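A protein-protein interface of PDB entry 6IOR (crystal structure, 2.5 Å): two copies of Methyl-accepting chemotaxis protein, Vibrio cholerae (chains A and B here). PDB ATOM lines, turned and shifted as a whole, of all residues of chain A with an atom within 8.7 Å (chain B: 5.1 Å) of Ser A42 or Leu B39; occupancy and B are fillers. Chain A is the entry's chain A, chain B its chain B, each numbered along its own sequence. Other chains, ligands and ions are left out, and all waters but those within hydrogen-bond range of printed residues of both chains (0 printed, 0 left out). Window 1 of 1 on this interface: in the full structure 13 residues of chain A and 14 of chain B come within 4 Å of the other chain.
Of the printed residues of chain B, Ser A42 touches Leu B39, Asn B65 and Leu B66.
Leu B39 touches just these residues of chain A: Leu A39 and Ser A42.
Of chain A, only Leu A39 and Asn A65 come within 4 Å of Gly B38.
No residue of chain A comes within 4 Å of Ala B40.
Of the printed residues of chain B, Gln A41 touches Asn B65 (3.7 Å).
Printed residues of chain B within 4 Å of Leu A39: Gly B38 (3.7 Å) and Leu B39 (3.7 Å).
The nearest residue of chain A that does not touch Leu B39 is Gly A38 (4.2 Å).
N of Asn B65 is in hydrogen-bond range of OE1 of Glu A45, at 2.9 Å.
O of Gly A38 is in hydrogen-bond range of ND2 of Asn B65 (3.2 Å).
The side-chain amide nitrogen (ND2) of Asn A65 sits at hydrogen-bond distance from the side-chain hydroxyl (OG) of Ser B42 (3.0 Å).
The backbone carbonyl oxygen (O) of Gly B38 lies within hydrogen-bond range of the side-chain amide nitrogen (ND2) of Asn A65 (3.3 Å).
The side-chain amide nitrogen of Asn B65 is in hydrogen-bond range of the side-chain hydroxyl of Ser A42.
Hydrophobic or aromatic side chains of chain B that line the printed part of chain A: Leu B39 and Leu B66.
Among the printed residues, no Asp or Glu carboxylate lies within 4 Å of a Lys or Arg side-chain nitrogen of the other chain.
The backbone carbonyl oxygen (O) of Asn B65 lies within hydrogen-bond range of the side-chain hydroxyl (OG) of Ser B69.
The side-chain hydroxyl (OG) of Ser A42 is in hydrogen-bond range of the backbone carbonyl oxygen (O) of Gly A38, 3.5 Å away.
The backbone carbonyl oxygen of Leu B39 is in hydrogen-bond range of the side-chain hydroxyl of Thr B43, at 3.2 Å.
The side-chain amide nitrogen of Gln A41 is in hydrogen-bond range of the side-chain carboxylate of Glu A45, at 3.0 Å.
The side-chain hydroxyl (OG1) of Thr A43 lies within hydrogen-bond range of the backbone carbonyl oxygen (O) of Leu A39 (2.9 Å).
O of Asn A65 lies within hydrogen-bond range of OG of Ser A69 (2.8 Å).
Leu A39 touches its own counterpart, Leu B39.
Ser A42 touches Leu B39, but with the chains exchanged Leu A39 does not touch Ser B42 (4.3 Å).
Ser A42 touches Asn B65, and with the chains exchanged Asn A65 touches Ser B42.
Ser A42 touches Leu B66, and with the chains exchanged Leu A66 touches Ser B42.
Positions printed for both chains: 35, 36, 37, 38, 39, 40, 41, 42, 43, 44, 65, 66 and 69.
Among the printed residues, pairs that only touch across the chains: Ser A42 with Leu B66, Leu A66 with Ser B42, Asn A65 with Gln B41, Gln A41 with Asn B65, Leu A39 with Gly B38, Leu A39 with Leu B39, Ser A35 with Ser B35 and Ser A42 with Leu B39.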
ATOM      1  N   ALA A  34     -13.766  -2.423  -2.495  1.00  0.00           N
ATOM      2  CA  ALA A  34     -15.056  -3.092  -2.362  1.00  0.00           C
ATOM      3  C   ALA A  34     -14.906  -4.352  -1.506  1.00  0.00           C
ATOM      4  O   ALA A  34     -15.769  -4.687  -0.701  1.00  0.00           O
ATOM      5  CB  ALA A  34     -15.619  -3.428  -3.730  1.00  0.00           C
ATOM      6  N   SER A  35     -13.785  -5.034  -1.676  1.00  0.00           N
ATOM      7  CA  SER A  35     -13.422  -6.163  -0.840  1.00  0.00           C
ATOM      8  C   SER A  35     -13.105  -5.724   0.602  1.00  0.00           C
ATOM      9  O   SER A  35     -13.672  -6.247   1.550  1.00  0.00           O
ATOM     10  CB  SER A  35     -12.241  -6.888  -1.483  1.00  0.00           C
ATOM     11  OG  SER A  35     -11.540  -7.659  -0.543  1.00  0.00           O
ATOM     12  N   LYS A  36     -12.216  -4.749   0.769  1.00  0.00           N
ATOM     13  CA  LYS A  36     -11.927  -4.186   2.093  1.00  0.00           C
ATOM     14  C   LYS A  36     -13.167  -3.616   2.828  1.00  0.00           C
ATOM     15  O   LYS A  36     -13.228  -3.627   4.065  1.00  0.00           O
ATOM     16  CB  LYS A  36     -10.877  -3.085   1.967  1.00  0.00           C
ATOM     17  CG  LYS A  36      -9.466  -3.555   1.664  1.00  0.00           C
ATOM     18  CD  LYS A  36      -8.603  -2.358   1.326  1.00  0.00           C
ATOM     19  CE  LYS A  36      -7.141  -2.615   1.640  1.00  0.00           C
ATOM     20  NZ  LYS A  36      -6.626  -3.794   0.900  1.00  0.00           N
ATOM     21  N   LYS A  37     -14.139  -3.108   2.068  1.00  0.00           N
ATOM     22  CA  LYS A  37     -15.404  -2.619   2.630  1.00  0.00           C
ATOM     23  C   LYS A  37     -16.209  -3.721   3.297  1.00  0.00           C
ATOM     24  O   LYS A  37     -16.873  -3.478   4.301  1.00  0.00           O
ATOM     25  CB  LYS A  37     -16.269  -1.976   1.554  1.00  0.00           C
ATOM     26  CG  LYS A  37     -16.054  -0.500   1.382  1.00  0.00           C
ATOM     27  CD  LYS A  37     -16.333  -0.098  -0.060  1.00  0.00           C
ATOM     28  CE  LYS A  37     -17.750   0.387  -0.258  1.00  0.00           C
ATOM     29  NZ  LYS A  37     -17.923   0.836  -1.657  1.00  0.00           N
ATOM     30  N   GLY A  38     -16.169  -4.921   2.718  1.00  0.00           N
ATOM     31  CA  GLY A  38     -16.883  -6.048   3.278  1.00  0.00           C
ATOM     32  C   GLY A  38     -16.213  -6.485   4.568  1.00  0.00           C
ATOM     33  O   GLY A  38     -16.863  -6.872   5.536  1.00  0.00           O
ATOM     34  N   LEU A  39     -14.889  -6.417   4.572  1.00  0.00           N
ATOM     35  CA  LEU A  39     -14.107  -6.756   5.750  1.00  0.00           C
ATOM     36  C   LEU A  39     -14.393  -5.785   6.895  1.00  0.00           C
ATOM     37  O   LEU A  39     -14.678  -6.212   8.009  1.00  0.00           O
ATOM     38  CB  LEU A  39     -12.615  -6.762   5.415  1.00  0.00           C
ATOM     39  CG  LEU A  39     -11.814  -7.920   5.997  1.00  0.00           C
ATOM     40  CD1 LEU A  39     -12.209  -9.230   5.332  1.00  0.00           C
ATOM     41  CD2 LEU A  39     -10.344  -7.662   5.842  1.00  0.00           C
ATOM     42  N   ALA A  40     -14.337  -4.483   6.609  1.00  0.00           N
ATOM     43  CA  ALA A  40     -14.592  -3.449   7.621  1.00  0.00           C
ATOM     44  C   ALA A  40     -16.036  -3.482   8.168  1.00  0.00           C
ATOM     45  O   ALA A  40     -16.240  -3.474   9.388  1.00  0.00           O
ATOM     46  CB  ALA A  40     -14.271  -2.081   7.057  1.00  0.00           C
ATOM     47  N   GLN A  41     -17.030  -3.532   7.280  1.00  0.00           N
ATOM     48  CA  GLN A  41     -18.429  -3.660   7.709  1.00  0.00           C
ATOM     49  C   GLN A  41     -18.685  -4.857   8.637  1.00  0.00           C
ATOM     50  O   GLN A  41     -19.352  -4.713   9.670  1.00  0.00           O
ATOM     51  CB  GLN A  41     -19.349  -3.768   6.502  1.00  0.00           C
ATOM     52  CG  GLN A  41     -20.809  -3.867   6.871  1.00  0.00           C
ATOM     53  CD  GLN A  41     -21.397  -2.557   7.383  1.00  0.00           C
ATOM     54  OE1 GLN A  41     -21.135  -1.479   6.839  1.00  0.00           O
ATOM     55  NE2 GLN A  41     -22.216  -2.649   8.426  1.00  0.00           N
ATOM     56  N   SER A  42     -18.159  -6.030   8.288  1.00  0.00           N
ATOM     57  CA  SER A  42     -18.359  -7.194   9.138  1.00  0.00           C
ATOM     58  C   SER A  42     -17.584  -7.068  10.447  1.00  0.00           C
ATOM     59  O   SER A  42     -18.093  -7.439  11.504  1.00  0.00           O
ATOM     60  CB  SER A  42     -17.963  -8.490   8.424  1.00  0.00           C
ATOM     61  OG  SER A  42     -18.933  -8.874   7.459  1.00  0.00           O
ATOM     62  N   THR A  43     -16.359  -6.558  10.388  1.00  0.00           N
ATOM     63  CA  THR A  43     -15.590  -6.368  11.614  1.00  0.00           C
ATOM     64  C   THR A  43     -16.351  -5.414  12.554  1.00  0.00           C
ATOM     65  O   THR A  43     -16.477  -5.657  13.763  1.00  0.00           O
ATOM     66  CB  THR A  43     -14.178  -5.821  11.331  1.00  0.00           C
ATOM     67  OG1 THR A  43     -13.451  -6.760  10.535  1.00  0.00           O
ATOM     68  CG2 THR A  43     -13.432  -5.644  12.612  1.00  0.00           C
ATOM     69  N   THR A  44     -16.892  -4.348  11.983  1.00  0.00           N
ATOM     70  CA  THR A  44     -17.651  -3.410  12.776  1.00  0.00           C
ATOM     71  C   THR A  44     -18.892  -4.058  13.384  1.00  0.00           C
ATOM     72  O   THR A  44     -19.227  -3.774  14.523  1.00  0.00           O
ATOM     73  CB  THR A  44     -18.058  -2.197  11.949  1.00  0.00           C
ATOM     74  OG1 THR A  44     -16.874  -1.585  11.429  1.00  0.00           O
ATOM     75  CG2 THR A  44     -18.821  -1.196  12.805  1.00  0.00           C
ATOM     76  N   GLU A  45     -19.559  -4.942  12.644  1.00  0.00           N
ATOM     77  CA  GLU A  45     -20.768  -5.570  13.161  1.00  0.00           C
ATOM     78  C   GLU A  45     -20.464  -6.547  14.296  1.00  0.00           C
ATOM     79  O   GLU A  45     -21.218  -6.634  15.271  1.00  0.00           O
ATOM     80  CB  GLU A  45     -21.526  -6.282  12.035  1.00  0.00           C
ATOM     81  CG  GLU A  45     -22.265  -5.327  11.116  1.00  0.00           C
ATOM     82  CD  GLU A  45     -22.921  -6.014   9.916  1.00  0.00           C
ATOM     83  OE1 GLU A  45     -22.875  -7.258   9.836  1.00  0.00           O
ATOM     84  OE2 GLU A  45     -23.474  -5.301   9.043  1.00  0.00           O
ATOM     85  N   ILE A  46     -19.363  -7.281  14.158  1.00  0.00           N
ATOM     86  CA  ILE A  46     -18.933  -8.244  15.166  1.00  0.00           C
ATOM     87  C   ILE A  46     -18.562  -7.534  16.474  1.00  0.00           C
ATOM     88  O   ILE A  46     -18.773  -8.064  17.565  1.00  0.00           O
ATOM     89  CB  ILE A  46     -17.736  -9.077  14.655  1.00  0.00           C
ATOM     90  CG1 ILE A  46     -18.216 -10.117  13.636  1.00  0.00           C
ATOM     91  CG2 ILE A  46     -16.980  -9.761  15.809  1.00  0.00           C
ATOM     92  CD1 ILE A  46     -17.070 -10.814  12.867  1.00  0.00           C
ATOM     93  N   LEU A  47     -18.002  -6.333  16.356  1.00  0.00           N
ATOM     94  CA  LEU A  47     -17.593  -5.595  17.533  1.00  0.00           C
ATOM     95  C   LEU A  47     -18.816  -5.054  18.291  1.00  0.00           C
ATOM     96  O   LEU A  47     -18.778  -4.944  19.504  1.00  0.00           O
ATOM     97  CB  LEU A  47     -16.624  -4.462  17.166  1.00  0.00           C
ATOM     98  CG  LEU A  47     -15.139  -4.826  16.985  1.00  0.00           C
ATOM     99  CD1 LEU A  47     -14.253  -3.591  16.965  1.00  0.00           C
ATOM    100  CD2 LEU A  47     -14.624  -5.784  18.037  1.00  0.00           C
ATOM    101  N   GLN A  48     -19.916  -4.763  17.602  1.00  0.00           N
ATOM    102  CA  GLN A  48     -21.088  -4.258  18.311  1.00  0.00           C
ATOM    103  C   GLN A  48     -21.774  -5.352  19.120  1.00  0.00           C
ATOM    104  O   GLN A  48     -22.768  -5.081  19.797  1.00  0.00           O
ATOM    105  CB  GLN A  48     -22.120  -3.631  17.372  1.00  0.00           C
ATOM    106  CG  GLN A  48     -21.612  -3.072  16.088  1.00  0.00           C
ATOM    107  CD  GLN A  48     -22.562  -2.083  15.443  1.00  0.00           C
ATOM    108  OE1 GLN A  48     -22.892  -1.034  15.995  1.00  0.00           O
ATOM    109  NE2 GLN A  48     -23.098  -2.482  14.301  1.00  0.00           N
ATOM    110  N   LEU A  49     -21.285  -6.584  19.022  1.00  0.00           N
ATOM    111  CA  LEU A  49     -21.709  -7.620  19.946  1.00  0.00           C
ATOM    112  C   LEU A  49     -21.355  -7.181  21.369  1.00  0.00           C
ATOM    113  O   LEU A  49     -22.088  -7.487  22.314  1.00  0.00           O
ATOM    114  CB  LEU A  49     -21.056  -8.959  19.602  1.00  0.00           C
ATOM    115  CG  LEU A  49     -21.600  -9.633  18.340  1.00  0.00           C
ATOM    116  CD1 LEU A  49     -20.783 -10.882  17.906  1.00  0.00           C
ATOM    117  CD2 LEU A  49     -23.067  -9.986  18.556  1.00  0.00           C
ATOM    118  N   PHE A  56     -11.860  -7.063  24.040  1.00  0.00           N
ATOM    119  CA  PHE A  56     -12.453  -7.698  22.870  1.00  0.00           C
ATOM    120  C   PHE A  56     -11.964  -7.007  21.594  1.00  0.00           C
ATOM    121  O   PHE A  56     -11.389  -7.636  20.691  1.00  0.00           O
ATOM    122  CB  PHE A  56     -13.984  -7.634  22.975  1.00  0.00           C
ATOM    123  CG  PHE A  56     -14.706  -8.252  21.815  1.00  0.00           C
ATOM    124  CD1 PHE A  56     -14.293  -9.468  21.289  1.00  0.00           C
ATOM    125  CD2 PHE A  56     -15.816  -7.629  21.268  1.00  0.00           C
ATOM    126  CE1 PHE A  56     -14.968 -10.041  20.234  1.00  0.00           C
ATOM    127  CE2 PHE A  56     -16.498  -8.197  20.208  1.00  0.00           C
ATOM    128  CZ  PHE A  56     -16.076  -9.403  19.689  1.00  0.00           C
ATOM    129  N   VAL A  60      -9.723  -8.609  18.367  1.00  0.00           N
ATOM    130  CA  VAL A  60     -10.208  -8.611  16.999  1.00  0.00           C
ATOM    131  C   VAL A  60      -9.286  -7.846  16.048  1.00  0.00           C
ATOM    132  O   VAL A  60      -8.977  -8.322  14.967  1.00  0.00           O
ATOM    133  CB  VAL A  60     -11.614  -8.015  16.940  1.00  0.00           C
ATOM    134  CG1 VAL A  60     -12.029  -7.749  15.490  1.00  0.00           C
ATOM    135  CG2 VAL A  60     -12.583  -8.942  17.653  1.00  0.00           C
ATOM    136  N   ASN A  65      -5.007 -11.850   9.674  1.00  0.00           N
ATOM    137  CA  ASN A  65      -5.462 -11.510   8.342  1.00  0.00           C
ATOM    138  C   ASN A  65      -6.019 -10.105   8.272  1.00  0.00           C
ATOM    139  O   ASN A  65      -5.722  -9.352   7.350  1.00  0.00           O
ATOM    140  CB  ASN A  65      -6.522 -12.483   7.857  1.00  0.00           C
ATOM    141  CG  ASN A  65      -6.842 -12.280   6.405  1.00  0.00           C
ATOM    142  OD1 ASN A  65      -6.004 -12.549   5.536  1.00  0.00           O
ATOM    143  ND2 ASN A  65      -8.040 -11.781   6.121  1.00  0.00           N
ATOM    144  N   LEU A  66      -6.847  -9.778   9.249  1.00  0.00           N
ATOM    145  CA  LEU A  66      -7.428  -8.460   9.380  1.00  0.00           C
ATOM    146  C   LEU A  66      -6.337  -7.403   9.495  1.00  0.00           C
ATOM    147  O   LEU A  66      -6.309  -6.425   8.729  1.00  0.00           O
ATOM    148  CB  LEU A  66      -8.351  -8.416  10.596  1.00  0.00           C
ATOM    149  CG  LEU A  66      -9.141  -7.119  10.670  1.00  0.00           C
ATOM    150  CD1 LEU A  66      -9.944  -6.928   9.367  1.00  0.00           C
ATOM    151  CD2 LEU A  66     -10.024  -7.083  11.903  1.00  0.00           C
ATOM    152  N   SER A  69      -4.591  -6.849   6.174  1.00  0.00           N
ATOM    153  CA  SER A  69      -5.344  -6.337   5.033  1.00  0.00           C
ATOM    154  C   SER A  69      -5.389  -4.816   4.976  1.00  0.00           C
ATOM    155  O   SER A  69      -5.899  -4.256   4.012  1.00  0.00           O
ATOM    156  CB  SER A  69      -6.781  -6.851   5.061  1.00  0.00           C
ATOM    157  OG  SER A  69      -6.847  -8.251   4.996  1.00  0.00           O
ATOM    158  N   LEU A 113     -21.161   2.961   6.903  1.00  0.00           N
ATOM    159  CA  LEU A 113     -19.842   2.841   6.296  1.00  0.00           C
ATOM    160  C   LEU A 113     -19.581   3.975   5.318  1.00  0.00           C
ATOM    161  O   LEU A 113     -20.447   4.366   4.528  1.00  0.00           O
ATOM    162  CB  LEU A 113     -19.694   1.505   5.582  1.00  0.00           C
ATOM    163  CG  LEU A 113     -18.272   1.068   5.245  1.00  0.00           C
ATOM    164  CD1 LEU A 113     -18.163  -0.454   5.370  1.00  0.00           C
ATOM    165  CD2 LEU A 113     -17.881   1.536   3.858  1.00  0.00           C
ATOM    166  N   THR A 133     -16.419   3.621   9.922  1.00  0.00           N
ATOM    167  CA  THR A 133     -17.701   3.058  10.350  1.00  0.00           C
ATOM    168  C   THR A 133     -18.163   3.593  11.702  1.00  0.00           C
ATOM    169  O   THR A 133     -17.362   3.769  12.608  1.00  0.00           O
ATOM    170  CB  THR A 133     -17.645   1.510  10.458  1.00  0.00           C
ATOM    171  OG1 THR A 133     -16.599   1.151  11.362  1.00  0.00           O
ATOM    172  CG2 THR A 133     -17.392   0.870   9.091  1.00  0.00           C
ATOM    173  N   MET A 145     -14.786   3.819  13.795  1.00  0.00           N
ATOM    174  CA  MET A 145     -13.555   3.148  13.394  1.00  0.00           C
ATOM    175  C   MET A 145     -12.922   3.719  12.132  1.00  0.00           C
ATOM    176  O   MET A 145     -13.608   4.249  11.262  1.00  0.00           O
ATOM    177  CB  MET A 145     -13.815   1.667  13.167  1.00  0.00           C
ATOM    178  CG  MET A 145     -14.525   0.989  14.316  1.00  0.00           C
ATOM    179  SD  MET A 145     -14.285  -0.780  14.257  1.00  0.00           S
ATOM    180  CE  MET A 145     -15.862  -1.290  14.899  1.00  0.00           C
ATOM    181  N   TYR A 147     -10.314   2.282   9.002  1.00  0.00           N
ATOM    182  CA  TYR A 147      -9.556   1.243   8.317  1.00  0.00           C
ATOM    183  C   TYR A 147      -8.726   1.931   7.225  1.00  0.00           C
ATOM    184  O   TYR A 147      -9.265   2.389   6.209  1.00  0.00           O
ATOM    185  CB  TYR A 147     -10.480   0.188   7.713  1.00  0.00           C
ATOM    186  CG  TYR A 147     -11.411  -0.494   8.693  1.00  0.00           C
ATOM    187  CD1 TYR A 147     -12.470   0.194   9.272  1.00  0.00           C
ATOM    188  CD2 TYR A 147     -11.240  -1.843   9.022  1.00  0.00           C
ATOM    189  CE1 TYR A 147     -13.331  -0.438  10.162  1.00  0.00           C
ATOM    190  CE2 TYR A 147     -12.090  -2.481   9.906  1.00  0.00           C
ATOM    191  CZ  TYR A 147     -13.136  -1.776  10.474  1.00  0.00           C
ATOM    192  OH  TYR A 147     -14.003  -2.399  11.343  1.00  0.00           O
ATOM    193  N   SER B  35     -12.155 -12.111  -2.692  1.00  0.00           N
ATOM    194  CA  SER B  35     -12.807 -11.284  -1.674  1.00  0.00           C
ATOM    195  C   SER B  35     -13.371 -12.136  -0.521  1.00  0.00           C
ATOM    196  O   SER B  35     -13.090 -11.870   0.648  1.00  0.00           O
ATOM    197  CB  SER B  35     -13.901 -10.432  -2.343  1.00  0.00           C
ATOM    198  OG  SER B  35     -14.704  -9.734  -1.419  1.00  0.00           O
ATOM    199  N   LYS B  36     -14.124 -13.185  -0.846  1.00  0.00           N
ATOM    200  CA  LYS B  36     -14.741 -14.025   0.181  1.00  0.00           C
ATOM    201  C   LYS B  36     -13.714 -14.794   1.015  1.00  0.00           C
ATOM    202  O   LYS B  36     -13.905 -15.008   2.217  1.00  0.00           O
ATOM    203  CB  LYS B  36     -15.734 -15.001  -0.451  1.00  0.00           C
ATOM    204  CG  LYS B  36     -16.953 -14.338  -1.065  1.00  0.00           C
ATOM    205  CD  LYS B  36     -17.933 -15.404  -1.529  1.00  0.00           C
ATOM    206  CE  LYS B  36     -18.889 -14.925  -2.625  1.00  0.00           C
ATOM    207  NZ  LYS B  36     -19.669 -13.708  -2.291  1.00  0.00           N
ATOM    208  N   LYS B  37     -12.630 -15.210   0.381  1.00  0.00           N
ATOM    209  CA  LYS B  37     -11.550 -15.888   1.081  1.00  0.00           C
ATOM    210  C   LYS B  37     -11.003 -15.005   2.203  1.00  0.00           C
ATOM    211  O   LYS B  37     -10.691 -15.496   3.285  1.00  0.00           O
ATOM    212  CB  LYS B  37     -10.434 -16.272   0.101  1.00  0.00           C
ATOM    213  CG  LYS B  37     -10.765 -17.511  -0.756  1.00  0.00           C
ATOM    214  CD  LYS B  37     -10.110 -17.482  -2.146  1.00  0.00           C
ATOM    215  CE  LYS B  37      -8.632 -17.871  -2.118  1.00  0.00           C
ATOM    216  NZ  LYS B  37      -8.225 -18.534  -3.395  1.00  0.00           N
ATOM    217  N   GLY B  38     -10.906 -13.699   1.942  1.00  0.00           N
ATOM    218  CA  GLY B  38     -10.441 -12.765   2.947  1.00  0.00           C
ATOM    219  C   GLY B  38     -11.417 -12.682   4.101  1.00  0.00           C
ATOM    220  O   GLY B  38     -11.026 -12.741   5.262  1.00  0.00           O
ATOM    221  N   LEU B  39     -12.697 -12.577   3.760  1.00  0.00           N
ATOM    222  CA  LEU B  39     -13.770 -12.543   4.739  1.00  0.00           C
ATOM    223  C   LEU B  39     -13.835 -13.828   5.559  1.00  0.00           C
ATOM    224  O   LEU B  39     -13.856 -13.779   6.785  1.00  0.00           O
ATOM    225  CB  LEU B  39     -15.104 -12.290   4.031  1.00  0.00           C
ATOM    226  CG  LEU B  39     -16.359 -12.028   4.860  1.00  0.00           C
ATOM    227  CD1 LEU B  39     -16.116 -10.962   5.924  1.00  0.00           C
ATOM    228  CD2 LEU B  39     -17.498 -11.610   3.937  1.00  0.00           C
ATOM    229  N   ALA B  40     -13.859 -14.973   4.883  1.00  0.00           N
ATOM    230  CA  ALA B  40     -13.926 -16.261   5.566  1.00  0.00           C
ATOM    231  C   ALA B  40     -12.690 -16.497   6.460  1.00  0.00           C
ATOM    232  O   ALA B  40     -12.780 -17.150   7.509  1.00  0.00           O
ATOM    233  CB  ALA B  40     -14.081 -17.394   4.544  1.00  0.00           C
ATOM    234  N   GLN B  41     -11.537 -15.966   6.055  1.00  0.00           N
ATOM    235  CA  GLN B  41     -10.309 -16.137   6.838  1.00  0.00           C
ATOM    236  C   GLN B  41     -10.353 -15.298   8.127  1.00  0.00           C
ATOM    237  O   GLN B  41      -9.960 -15.764   9.194  1.00  0.00           O
ATOM    238  CB  GLN B  41      -9.082 -15.770   6.001  1.00  0.00           C
ATOM    239  CG  GLN B  41      -7.760 -15.780   6.768  1.00  0.00           C
ATOM    240  CD  GLN B  41      -7.283 -17.178   7.098  1.00  0.00           C
ATOM    241  OE1 GLN B  41      -7.514 -18.127   6.343  1.00  0.00           O
ATOM    242  NE2 GLN B  41      -6.615 -17.317   8.233  1.00  0.00           N
ATOM    243  N   SER B  42     -10.858 -14.071   8.040  1.00  0.00           N
ATOM    244  CA  SER B  42     -11.013 -13.266   9.247  1.00  0.00           C
ATOM    245  C   SER B  42     -12.165 -13.737  10.129  1.00  0.00           C
ATOM    246  O   SER B  42     -12.122 -13.556  11.331  1.00  0.00           O
ATOM    247  CB  SER B  42     -11.199 -11.797   8.898  1.00  0.00           C
ATOM    248  OG  SER B  42      -9.988 -11.279   8.373  1.00  0.00           O
ATOM    249  N   THR B  43     -13.202 -14.330   9.550  1.00  0.00           N
ATOM    250  CA  THR B  43     -14.290 -14.813  10.385  1.00  0.00           C
ATOM    251  C   THR B  43     -13.764 -15.966  11.209  1.00  0.00           C
ATOM    252  O   THR B  43     -14.000 -16.069  12.411  1.00  0.00           O
ATOM    253  CB  THR B  43     -15.501 -15.265   9.565  1.00  0.00           C
ATOM    254  OG1 THR B  43     -16.139 -14.117   8.991  1.00  0.00           O
ATOM    255  CG2 THR B  43     -16.516 -16.023  10.455  1.00  0.00           C
ATOM    256  N   THR B  44     -13.012 -16.821  10.551  1.00  0.00           N
ATOM    257  CA  THR B  44     -12.439 -17.958  11.225  1.00  0.00           C
ATOM    258  C   THR B  44     -11.490 -17.504  12.335  1.00  0.00           C
ATOM    259  O   THR B  44     -11.659 -17.936  13.469  1.00  0.00           O
ATOM    260  CB  THR B  44     -11.730 -18.889  10.216  1.00  0.00           C
ATOM    261  OG1 THR B  44     -12.671 -19.270   9.205  1.00  0.00           O
ATOM    262  CG2 THR B  44     -11.187 -20.139  10.895  1.00  0.00           C
ATOM    263  N   ASN B  65     -24.006  -8.327   7.337  1.00  0.00           N
ATOM    264  CA  ASN B  65     -23.102  -8.317   6.199  1.00  0.00           C
ATOM    265  C   ASN B  65     -22.465  -9.694   5.891  1.00  0.00           C
ATOM    266  O   ASN B  65     -22.386 -10.097   4.734  1.00  0.00           O
ATOM    267  CB  ASN B  65     -22.014  -7.286   6.405  1.00  0.00           C
ATOM    268  CG  ASN B  65     -21.154  -7.134   5.189  1.00  0.00           C
ATOM    269  OD1 ASN B  65     -21.558  -6.500   4.215  1.00  0.00           O
ATOM    270  ND2 ASN B  65     -19.967  -7.735   5.217  1.00  0.00           N
ATOM    271  N   LEU B  66     -22.034 -10.415   6.920  1.00  0.00           N
ATOM    272  CA  LEU B  66     -21.480 -11.757   6.744  1.00  0.00           C
ATOM    273  C   LEU B  66     -22.548 -12.739   6.251  1.00  0.00           C
ATOM    274  O   LEU B  66     -22.311 -13.537   5.346  1.00  0.00           O
ATOM    275  CB  LEU B  66     -20.861 -12.236   8.054  1.00  0.00           C
ATOM    276  CG  LEU B  66     -20.193 -13.597   8.214  1.00  0.00           C
ATOM    277  CD1 LEU B  66     -19.133 -13.838   7.143  1.00  0.00           C
ATOM    278  CD2 LEU B  66     -19.567 -13.717   9.619  1.00  0.00           C
ATOM    279  N   SER B  69     -23.237 -12.548   2.567  1.00  0.00           N
ATOM    280  CA  SER B  69     -22.063 -12.633   1.698  1.00  0.00           C
ATOM    281  C   SER B  69     -21.886 -14.049   1.187  1.00  0.00           C
ATOM    282  O   SER B  69     -21.126 -14.309   0.253  1.00  0.00           O
ATOM    283  CB  SER B  69     -20.794 -12.191   2.435  1.00  0.00           C
ATOM    284  OG  SER B  69     -20.860 -10.829   2.802  1.00  0.00           O
ATOM    285  N   PHE B  70     -22.599 -14.960   1.825  1.00  0.00           N
ATOM    286  CA  PHE B  70     -22.485 -16.359   1.506  1.00  0.00           C
ATOM    287  C   PHE B  70     -23.874 -16.958   1.407  1.00  0.00           C
ATOM    288  O   PHE B  70     -24.840 -16.399   1.932  1.00  0.00           O
ATOM    289  CB  PHE B  70     -21.632 -17.066   2.561  1.00  0.00           C
ATOM    290  CG  PHE B  70     -20.203 -16.571   2.603  1.00  0.00           C
ATOM    291  CD1 PHE B  70     -19.239 -17.119   1.766  1.00  0.00           C
ATOM    292  CD2 PHE B  70     -19.831 -15.540   3.460  1.00  0.00           C
ATOM    293  CE1 PHE B  70     -17.924 -16.665   1.793  1.00  0.00           C
ATOM    294  CE2 PHE B  70     -18.524 -15.083   3.495  1.00  0.00           C
ATOM    295  CZ  PHE B  70     -17.561 -15.650   2.650  1.00  0.00           C
